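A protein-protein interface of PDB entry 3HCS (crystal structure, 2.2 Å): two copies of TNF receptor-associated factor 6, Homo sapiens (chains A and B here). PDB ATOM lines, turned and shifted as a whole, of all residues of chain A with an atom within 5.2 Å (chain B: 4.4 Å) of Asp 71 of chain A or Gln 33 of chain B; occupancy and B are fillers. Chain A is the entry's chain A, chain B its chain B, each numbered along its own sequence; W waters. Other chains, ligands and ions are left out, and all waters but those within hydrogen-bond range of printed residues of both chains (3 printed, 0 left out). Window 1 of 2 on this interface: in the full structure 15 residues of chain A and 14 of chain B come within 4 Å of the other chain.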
ATOM      1  N   ALA A  31      26.459  23.014  31.883  1.00  0.00           N
ATOM      2  CA  ALA A  31      27.721  22.310  32.018  1.00  0.00           C
ATOM      3  C   ALA A  31      28.501  22.121  30.718  1.00  0.00           C
ATOM      4  O   ALA A  31      27.950  21.719  29.694  1.00  0.00           O
ATOM      5  CB  ALA A  31      27.466  20.950  32.663  1.00  0.00           C
ATOM      6  N   VAL A  32      29.788  22.436  30.769  1.00  0.00           N
ATOM      7  CA  VAL A  32      30.675  22.242  29.630  1.00  0.00           C
ATOM      8  C   VAL A  32      31.915  21.527  30.166  1.00  0.00           C
ATOM      9  O   VAL A  32      32.256  21.674  31.344  1.00  0.00           O
ATOM     10  CB  VAL A  32      31.093  23.586  28.984  1.00  0.00           C
ATOM     11  CG1 VAL A  32      29.869  24.285  28.419  1.00  0.00           C
ATOM     12  CG2 VAL A  32      31.790  24.473  30.010  1.00  0.00           C
ATOM     13  N   GLN A  33      32.571  20.747  29.315  1.00  0.00           N
ATOM     14  CA  GLN A  33      33.765  20.019  29.723  1.00  0.00           C
ATOM     15  C   GLN A  33      34.979  20.461  28.913  1.00  0.00           C
ATOM     16  O   GLN A  33      34.864  20.792  27.729  1.00  0.00           O
ATOM     17  CB  GLN A  33      33.556  18.517  29.541  1.00  0.00           C
ATOM     18  CG  GLN A  33      34.647  17.668  30.183  1.00  0.00           C
ATOM     19  CD  GLN A  33      34.399  16.186  30.005  1.00  0.00           C
ATOM     20  OE1 GLN A  33      33.272  15.711  30.170  1.00  0.00           O
ATOM     21  NE2 GLN A  33      35.450  15.443  29.672  1.00  0.00           N
ATOM     22  N   ARG A  39      34.788  19.806  34.436  1.00  0.00           N
ATOM     23  CA  ARG A  39      33.490  20.416  34.186  1.00  0.00           C
ATOM     24  C   ARG A  39      33.330  21.776  34.834  1.00  0.00           C
ATOM     25  O   ARG A  39      33.799  21.999  35.945  1.00  0.00           O
ATOM     26  CB  ARG A  39      32.385  19.509  34.703  1.00  0.00           C
ATOM     27  CG  ARG A  39      32.336  18.144  34.076  1.00  0.00           C
ATOM     28  CD  ARG A  39      31.550  17.262  35.006  1.00  0.00           C
ATOM     29  NE  ARG A  39      30.933  16.131  34.342  1.00  0.00           N
ATOM     30  CZ  ARG A  39      30.171  15.252  34.976  1.00  0.00           C
ATOM     31  NH1 ARG A  39      29.954  15.394  36.277  1.00  0.00           N
ATOM     32  NH2 ARG A  39      29.623  14.242  34.313  1.00  0.00           N
ATOM     33  N   PHE A  69      33.277  21.642  25.272  1.00  0.00           N
ATOM     34  CA  PHE A  69      32.180  20.930  24.653  1.00  0.00           C
ATOM     35  C   PHE A  69      31.031  20.849  25.653  1.00  0.00           C
ATOM     36  O   PHE A  69      31.243  20.777  26.866  1.00  0.00           O
ATOM     37  CB  PHE A  69      32.648  19.578  24.058  1.00  0.00           C
ATOM     38  CG  PHE A  69      32.533  18.386  24.965  1.00  0.00           C
ATOM     39  CD1 PHE A  69      31.290  17.850  25.300  1.00  0.00           C
ATOM     40  CD2 PHE A  69      33.683  17.712  25.380  1.00  0.00           C
ATOM     41  CE1 PHE A  69      31.191  16.659  26.026  1.00  0.00           C
ATOM     42  CE2 PHE A  69      33.593  16.522  26.106  1.00  0.00           C
ATOM     43  CZ  PHE A  69      32.345  15.994  26.427  1.00  0.00           C
ATOM     44  N   PRO A  70      29.787  20.953  25.158  1.00  0.00           N
ATOM     45  CA  PRO A  70      28.631  20.894  26.057  1.00  0.00           C
ATOM     46  C   PRO A  70      28.465  19.521  26.681  1.00  0.00           C
ATOM     47  O   PRO A  70      28.284  18.534  25.973  1.00  0.00           O
ATOM     48  CB  PRO A  70      27.462  21.281  25.143  1.00  0.00           C
ATOM     49  CG  PRO A  70      27.882  20.727  23.813  1.00  0.00           C
ATOM     50  CD  PRO A  70      29.361  21.099  23.752  1.00  0.00           C
ATOM     51  N   ASP A  71      28.529  19.461  28.006  1.00  0.00           N
ATOM     52  CA  ASP A  71      28.386  18.189  28.688  1.00  0.00           C
ATOM     53  C   ASP A  71      26.916  17.980  28.968  1.00  0.00           C
ATOM     54  O   ASP A  71      26.429  18.217  30.071  1.00  0.00           O
ATOM     55  CB  ASP A  71      29.156  18.178  29.994  1.00  0.00           C
ATOM     56  CG  ASP A  71      29.405  16.774  30.485  1.00  0.00           C
ATOM     57  OD1 ASP A  71      28.475  15.945  30.383  1.00  0.00           O
ATOM     58  OD2 ASP A  71      30.524  16.500  30.966  1.00  0.00           O
ATOM     59  N   ASN A  72      26.196  17.554  27.947  1.00  0.00           N
ATOM     60  CA  ASN A  72      24.768  17.334  28.091  1.00  0.00           C
ATOM     61  C   ASN A  72      24.454  16.137  28.982  1.00  0.00           C
ATOM     62  O   ASN A  72      23.347  16.031  29.515  1.00  0.00           O
ATOM     63  CB  ASN A  72      24.106  17.175  26.710  1.00  0.00           C
ATOM     64  CG  ASN A  72      24.059  18.486  25.934  1.00  0.00           C
ATOM     65  OD1 ASN A  72      23.679  19.518  26.482  1.00  0.00           O
ATOM     66  ND2 ASN A  72      24.438  18.450  24.659  1.00  0.00           N
ATOM     67  N   PHE A  73      25.414  15.235  29.153  1.00  0.00           N
ATOM     68  CA  PHE A  73      25.148  14.106  30.023  1.00  0.00           C
ATOM     69  C   PHE A  73      25.032  14.665  31.446  1.00  0.00           C
ATOM     70  O   PHE A  73      24.090  14.344  32.167  1.00  0.00           O
ATOM     71  CB  PHE A  73      26.270  13.069  29.966  1.00  0.00           C
ATOM     72  CG  PHE A  73      26.004  11.858  30.821  1.00  0.00           C
ATOM     73  CD1 PHE A  73      25.306  10.771  30.310  1.00  0.00           C
ATOM     74  CD2 PHE A  73      26.398  11.835  32.157  1.00  0.00           C
ATOM     75  CE1 PHE A  73      24.998   9.671  31.118  1.00  0.00           C
ATOM     76  CE2 PHE A  73      26.099  10.745  32.975  1.00  0.00           C
ATOM     77  CZ  PHE A  73      25.397   9.661  32.456  1.00  0.00           C
ATOM     78  N   ALA A  74      25.987  15.515  31.822  1.00  0.00           N
ATOM     79  CA  ALA A  74      26.015  16.123  33.157  1.00  0.00           C
ATOM     80  C   ALA A  74      24.794  17.003  33.389  1.00  0.00           C
ATOM     81  O   ALA A  74      24.200  16.993  34.471  1.00  0.00           O
ATOM     82  CB  ALA A  74      27.289  16.956  33.327  1.00  0.00           C
ATOM     83  N   LYS A  75      24.433  17.775  32.369  1.00  0.00           N
ATOM     84  CA  LYS A  75      23.281  18.664  32.467  1.00  0.00           C
ATOM     85  C   LYS A  75      22.021  17.860  32.772  1.00  0.00           C
ATOM     86  O   LYS A  75      21.285  18.177  33.702  1.00  0.00           O
ATOM     87  CB  LYS A  75      23.108  19.462  31.167  1.00  0.00           C
ATOM     88  CG  LYS A  75      21.934  20.430  31.186  1.00  0.00           C
ATOM     89  CD  LYS A  75      21.844  21.236  29.901  1.00  0.00           C
ATOM     90  CE  LYS A  75      20.566  22.065  29.871  1.00  0.00           C
ATOM     91  NZ  LYS A  75      20.433  22.873  28.622  1.00  0.00           N
ATOM     92  N   VAL B  32      33.492   8.438  25.237  1.00  0.00           N
ATOM     93  CA  VAL B  32      33.236   9.571  24.358  1.00  0.00           C
ATOM     94  C   VAL B  32      31.770   9.951  24.536  1.00  0.00           C
ATOM     95  O   VAL B  32      30.934   9.097  24.861  1.00  0.00           O
ATOM     96  CB  VAL B  32      33.479   9.226  22.877  1.00  0.00           C
ATOM     97  CG1 VAL B  32      34.935   8.855  22.668  1.00  0.00           C
ATOM     98  CG2 VAL B  32      32.570   8.094  22.452  1.00  0.00           C
ATOM     99  N   GLN B  33      31.458  11.229  24.340  1.00  0.00           N
ATOM    100  CA  GLN B  33      30.077  11.693  24.481  1.00  0.00           C
ATOM    101  C   GLN B  33      29.534  12.256  23.162  1.00  0.00           C
ATOM    102  O   GLN B  33      30.256  12.897  22.397  1.00  0.00           O
ATOM    103  CB  GLN B  33      29.974  12.763  25.587  1.00  0.00           C
ATOM    104  CG  GLN B  33      28.577  12.871  26.205  1.00  0.00           C
ATOM    105  CD  GLN B  33      28.459  13.968  27.270  1.00  0.00           C
ATOM    106  OE1 GLN B  33      29.269  14.046  28.201  1.00  0.00           O
ATOM    107  NE2 GLN B  33      27.441  14.813  27.134  1.00  0.00           N
ATOM    108  N   THR B  34      28.249  12.018  22.924  1.00  0.00           N
ATOM    109  CA  THR B  34      27.553  12.471  21.726  1.00  0.00           C
ATOM    110  C   THR B  34      26.906  13.837  21.957  1.00  0.00           C
ATOM    111  O   THR B  34      26.734  14.267  23.098  1.00  0.00           O
ATOM    112  CB  THR B  34      26.442  11.483  21.344  1.00  0.00           C
ATOM    113  OG1 THR B  34      25.449  11.457  22.381  1.00  0.00           O
ATOM    114  CG2 THR B  34      27.012  10.092  21.162  1.00  0.00           C
ATOM    115  N   PRO B  35      26.507  14.526  20.872  1.00  0.00           N
ATOM    116  CA  PRO B  35      25.874  15.848  20.994  1.00  0.00           C
ATOM    117  C   PRO B  35      24.577  15.736  21.784  1.00  0.00           C
ATOM    118  O   PRO B  35      24.163  16.663  22.484  1.00  0.00           O
ATOM    119  CB  PRO B  35      25.602  16.247  19.544  1.00  0.00           C
ATOM    120  CG  PRO B  35      26.603  15.440  18.753  1.00  0.00           C
ATOM    121  CD  PRO B  35      26.581  14.108  19.463  1.00  0.00           C
ATOM    122  N   GLY B  37      24.071  14.073  24.338  1.00  0.00           N
ATOM    123  CA  GLY B  37      24.346  13.715  25.721  1.00  0.00           C
ATOM    124  C   GLY B  37      24.436  12.264  26.164  1.00  0.00           C
ATOM    125  O   GLY B  37      24.101  11.956  27.312  1.00  0.00           O
ATOM    126  N   HIS B  38      24.887  11.369  25.289  1.00  0.00           N
ATOM    127  CA  HIS B  38      25.030   9.970  25.670  1.00  0.00           C
ATOM    128  C   HIS B  38      26.481   9.499  25.578  1.00  0.00           C
ATOM    129  O   HIS B  38      27.193   9.826  24.634  1.00  0.00           O
ATOM    130  CB  HIS B  38      24.114   9.076  24.825  1.00  0.00           C
ATOM    131  CG  HIS B  38      22.673   9.157  25.224  1.00  0.00           C
ATOM    132  ND1 HIS B  38      21.751   9.924  24.543  1.00  0.00           N
ATOM    133  CD2 HIS B  38      22.009   8.615  26.272  1.00  0.00           C
ATOM    134  CE1 HIS B  38      20.581   9.849  25.154  1.00  0.00           C
ATOM    135  NE2 HIS B  38      20.712   9.061  26.207  1.00  0.00           N
ATOM    136  N   ARG B  39      26.908   8.747  26.586  1.00  0.00           N
ATOM    137  CA  ARG B  39      28.271   8.224  26.663  1.00  0.00           C
ATOM    138  C   ARG B  39      28.377   6.820  26.083  1.00  0.00           C
ATOM    139  O   ARG B  39      27.459   6.016  26.214  1.00  0.00           O
ATOM    140  CB  ARG B  39      28.732   8.159  28.119  1.00  0.00           C
ATOM    141  CG  ARG B  39      28.830   9.475  28.842  1.00  0.00           C
ATOM    142  CD  ARG B  39      28.978   9.232  30.337  1.00  0.00           C
ATOM    143  NE  ARG B  39      29.380  10.434  31.059  1.00  0.00           N
ATOM    144  CZ  ARG B  39      29.424  10.526  32.384  1.00  0.00           C
ATOM    145  NH1 ARG B  39      29.085   9.489  33.136  1.00  0.00           N
ATOM    146  NH2 ARG B  39      29.814  11.653  32.958  1.00  0.00           N
ATOM    147  N   GLN B  67      31.523  14.199  15.360  1.00  0.00           N
ATOM    148  CA  GLN B  67      30.769  14.977  16.340  1.00  0.00           C
ATOM    149  C   GLN B  67      31.020  14.511  17.773  1.00  0.00           C
ATOM    150  O   GLN B  67      30.648  15.199  18.726  1.00  0.00           O
ATOM    151  CB  GLN B  67      29.259  14.913  16.052  1.00  0.00           C
ATOM    152  CG  GLN B  67      28.801  15.652  14.799  1.00  0.00           C
ATOM    153  CD  GLN B  67      27.294  15.570  14.585  1.00  0.00           C
ATOM    154  OE1 GLN B  67      26.705  14.487  14.615  1.00  0.00           O
ATOM    155  NE2 GLN B  67      26.666  16.715  14.356  1.00  0.00           N
ATOM    156  N   LEU B  68      31.641  13.343  17.916  1.00  0.00           N
ATOM    157  CA  LEU B  68      31.950  12.784  19.224  1.00  0.00           C
ATOM    158  C   LEU B  68      33.049  13.584  19.910  1.00  0.00           C
ATOM    159  O   LEU B  68      33.908  14.163  19.256  1.00  0.00           O
ATOM    160  CB  LEU B  68      32.407  11.339  19.078  1.00  0.00           C
ATOM    161  CG  LEU B  68      31.406  10.381  18.447  1.00  0.00           C
ATOM    162  CD1 LEU B  68      32.099   9.065  18.155  1.00  0.00           C
ATOM    163  CD2 LEU B  68      30.222  10.183  19.380  1.00  0.00           C
ATOM    164  N   PHE B  69      33.009  13.622  21.235  1.00  0.00           N
ATOM    165  CA  PHE B  69      34.007  14.333  22.024  1.00  0.00           C
ATOM    166  C   PHE B  69      34.540  13.395  23.106  1.00  0.00           C
ATOM    167  O   PHE B  69      33.777  12.639  23.719  1.00  0.00           O
ATOM    168  CB  PHE B  69      33.363  15.535  22.722  1.00  0.00           C
ATOM    169  CG  PHE B  69      33.575  16.842  22.018  1.00  0.00           C
ATOM    170  CD1 PHE B  69      34.824  17.466  22.038  1.00  0.00           C
ATOM    171  CD2 PHE B  69      32.525  17.464  21.342  1.00  0.00           C
ATOM    172  CE1 PHE B  69      35.026  18.695  21.396  1.00  0.00           C
ATOM    173  CE2 PHE B  69      32.717  18.693  20.695  1.00  0.00           C
ATOM    174  CZ  PHE B  69      33.972  19.307  20.725  1.00  0.00           C
ATOM    175  N   ASP B  71      35.205  12.116  26.494  1.00  0.00           N
ATOM    176  CA  ASP B  71      34.677  12.467  27.810  1.00  0.00           C
ATOM    177  C   ASP B  71      35.727  12.078  28.831  1.00  0.00           C
ATOM    178  O   ASP B  71      35.586  11.069  29.520  1.00  0.00           O
ATOM    179  CB  ASP B  71      33.368  11.716  28.102  1.00  0.00           C
ATOM    180  CG  ASP B  71      32.596  12.306  29.298  1.00  0.00           C
ATOM    181  OD1 ASP B  71      33.219  12.857  30.232  1.00  0.00           O
ATOM    182  OD2 ASP B  71      31.351  12.203  29.311  1.00  0.00           O
HETATM  183  O   HOH W   1      30.453  13.749  31.515  1.00  0.00           O
HETATM  184  O   HOH W   2      29.050  11.751  35.961  1.00  0.00           O
HETATM  185  O   HOH W   3      26.622  16.607  25.236  1.00  0.00           O
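Water W1 lies within hydrogen-bond range of NH2 of Arg 39 of chain B (2.6 Å), OD2 of Asp 71 of chain A (2.8 Å), OD2 of Asp 71 of chain B (2.8 Å) and NH2 of Arg 39 of chain A (3.0 Å). Water W3 lies within hydrogen-bond range of the backbone carbonyl oxygen of Pro 70 of chain A, the side-chain amide nitrogen of Gln 33 of chain B, the backbone NH of Asn 72 of chain A and the backbone carbonyl oxygen of Thr 34 of chain B. Water W2 lies within hydrogen-bond range of NH2 of Arg 39 of chain A (3.0 Å) and NH2 of Arg 39 of chain B (3.1 Å).
OD1 of Asp 71 of chain B lies close to OE1 of Gln 33 of chain A. OD1 of Asp 71 of chain A lies close to OE1 of Gln 33 of chain B (3.0 Å). The side-chain amide nitrogen (NE2) of Gln 33 of chain B sits close to the backbone NH (N) of Asn 72 of chain A, at 3.1 Å. The backbone carbonyl oxygen (O) of Pro 35 of chain B is in hydrogen-bond range of the side-chain amide nitrogen (ND2) of Asn 72 of chain A, at 2.8 Å. The side-chain amide nitrogen (NE2) of Gln 33 of chain B lies close to the backbone NH (N) of Phe 73 of chain A (2.9 Å). The guanidinium group (NH2) of Arg 39 of chain A sits close to the guanidinium group (NH2) of Arg 39 of chain B (2.9 Å).
Printed residues of chain B that touch a printed residue of chain A: Gln 33, Pro 35, Gly 37, Arg 39, Phe 69 and Asp 71. Hydrophobic or aromatic side chains of chain B that line the printed part of chain A: Phe 69. Among the printed residues, 12 pairs touch across the chains. Among the printed residues, no Asp or Glu carboxylate lies within 4 Å of a Lys or Arg side-chain nitrogen of the other chain.
The backbone NH (N) of Gln 33 of chain A sits at hydrogen-bond distance from the backbone carbonyl oxygen (O) of Phe 69 of chain A, 2.8 Å away. The side-chain carboxylate (OD1) of Asp 71 of chain A sits close to the backbone NH (N) of Phe 73 of chain A (3.4 Å). OD1 of Asp 71 of chain A lies within hydrogen-bond range of N of Ala 74 of chain A, 2.9 Å away. The backbone carbonyl oxygen of Phe 69 of chain B sits at hydrogen-bond distance from the backbone NH of Gln 33 of chain B (2.8 Å). The side-chain amide oxygen (OE1) of Gln 33 of chain B sits close to the side-chain carboxylate (OD2) of Asp 71 of chain B, at 3.0 Å. OD2 of Asp 71 of chain B lies within salt-bridge range of NE of Arg 39 of chain B, at 3.2 Å.
Among the printed residues, merely in contact across the chains: Phe 69 of chain A with Gln 33 of chain B (3.9 Å), Phe 69 of chain A with Phe 69 of chain B (3.4 Å), Pro 70 of chain A with Gln 33 of chain B (3.99 Å), Asn 72 of chain A with Gly 37 of chain B (3.6 Å), Phe 73 of chain A with Gly 37 of chain B (3.4 Å) and Phe 73 of chain A with Arg 39 of chain B (3.2 Å).
Asp 71 of chain A touches just one residue of chain B: Gln 33 (3.0 Å). Of the printed residues of chain A, Pro 35 of chain B touches Asn 72 (2.8 Å). Printed residues of chain B within 4 Å of Pro 70 of chain A: Gln 33 (3.99 Å). Of the printed residues of chain B, Gln 33 of chain A touches Asp 71. Lys 75 of chain A touches none of the printed residues of chain B. Val 32 of chain B touches none of the printed residues of chain A. The nearest printed residue of chain B that does not touch Asp 71 of chain A is Asp 71 of chain B (4.6 Å). The nearest printed residue of chain A that does not touch Gln 33 of chain B is Gln 33 of chain A (4.8 Å).
Gln 33 of chain A touches Asp 71 of chain B, and with the chains exchanged Asp 71 of chain A touches Gln 33 of chain B. Arg 39 of chain B touches its own counterpart, Arg 39 of chain A. Phe 69 of chain A touches Gln 33 of chain B, but with the chains exchanged Gln 33 of chain A does not touch Phe 69 of chain B (6.6 Å). Phe 69 of chain B touches its own counterpart, Phe 69 of chain A.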
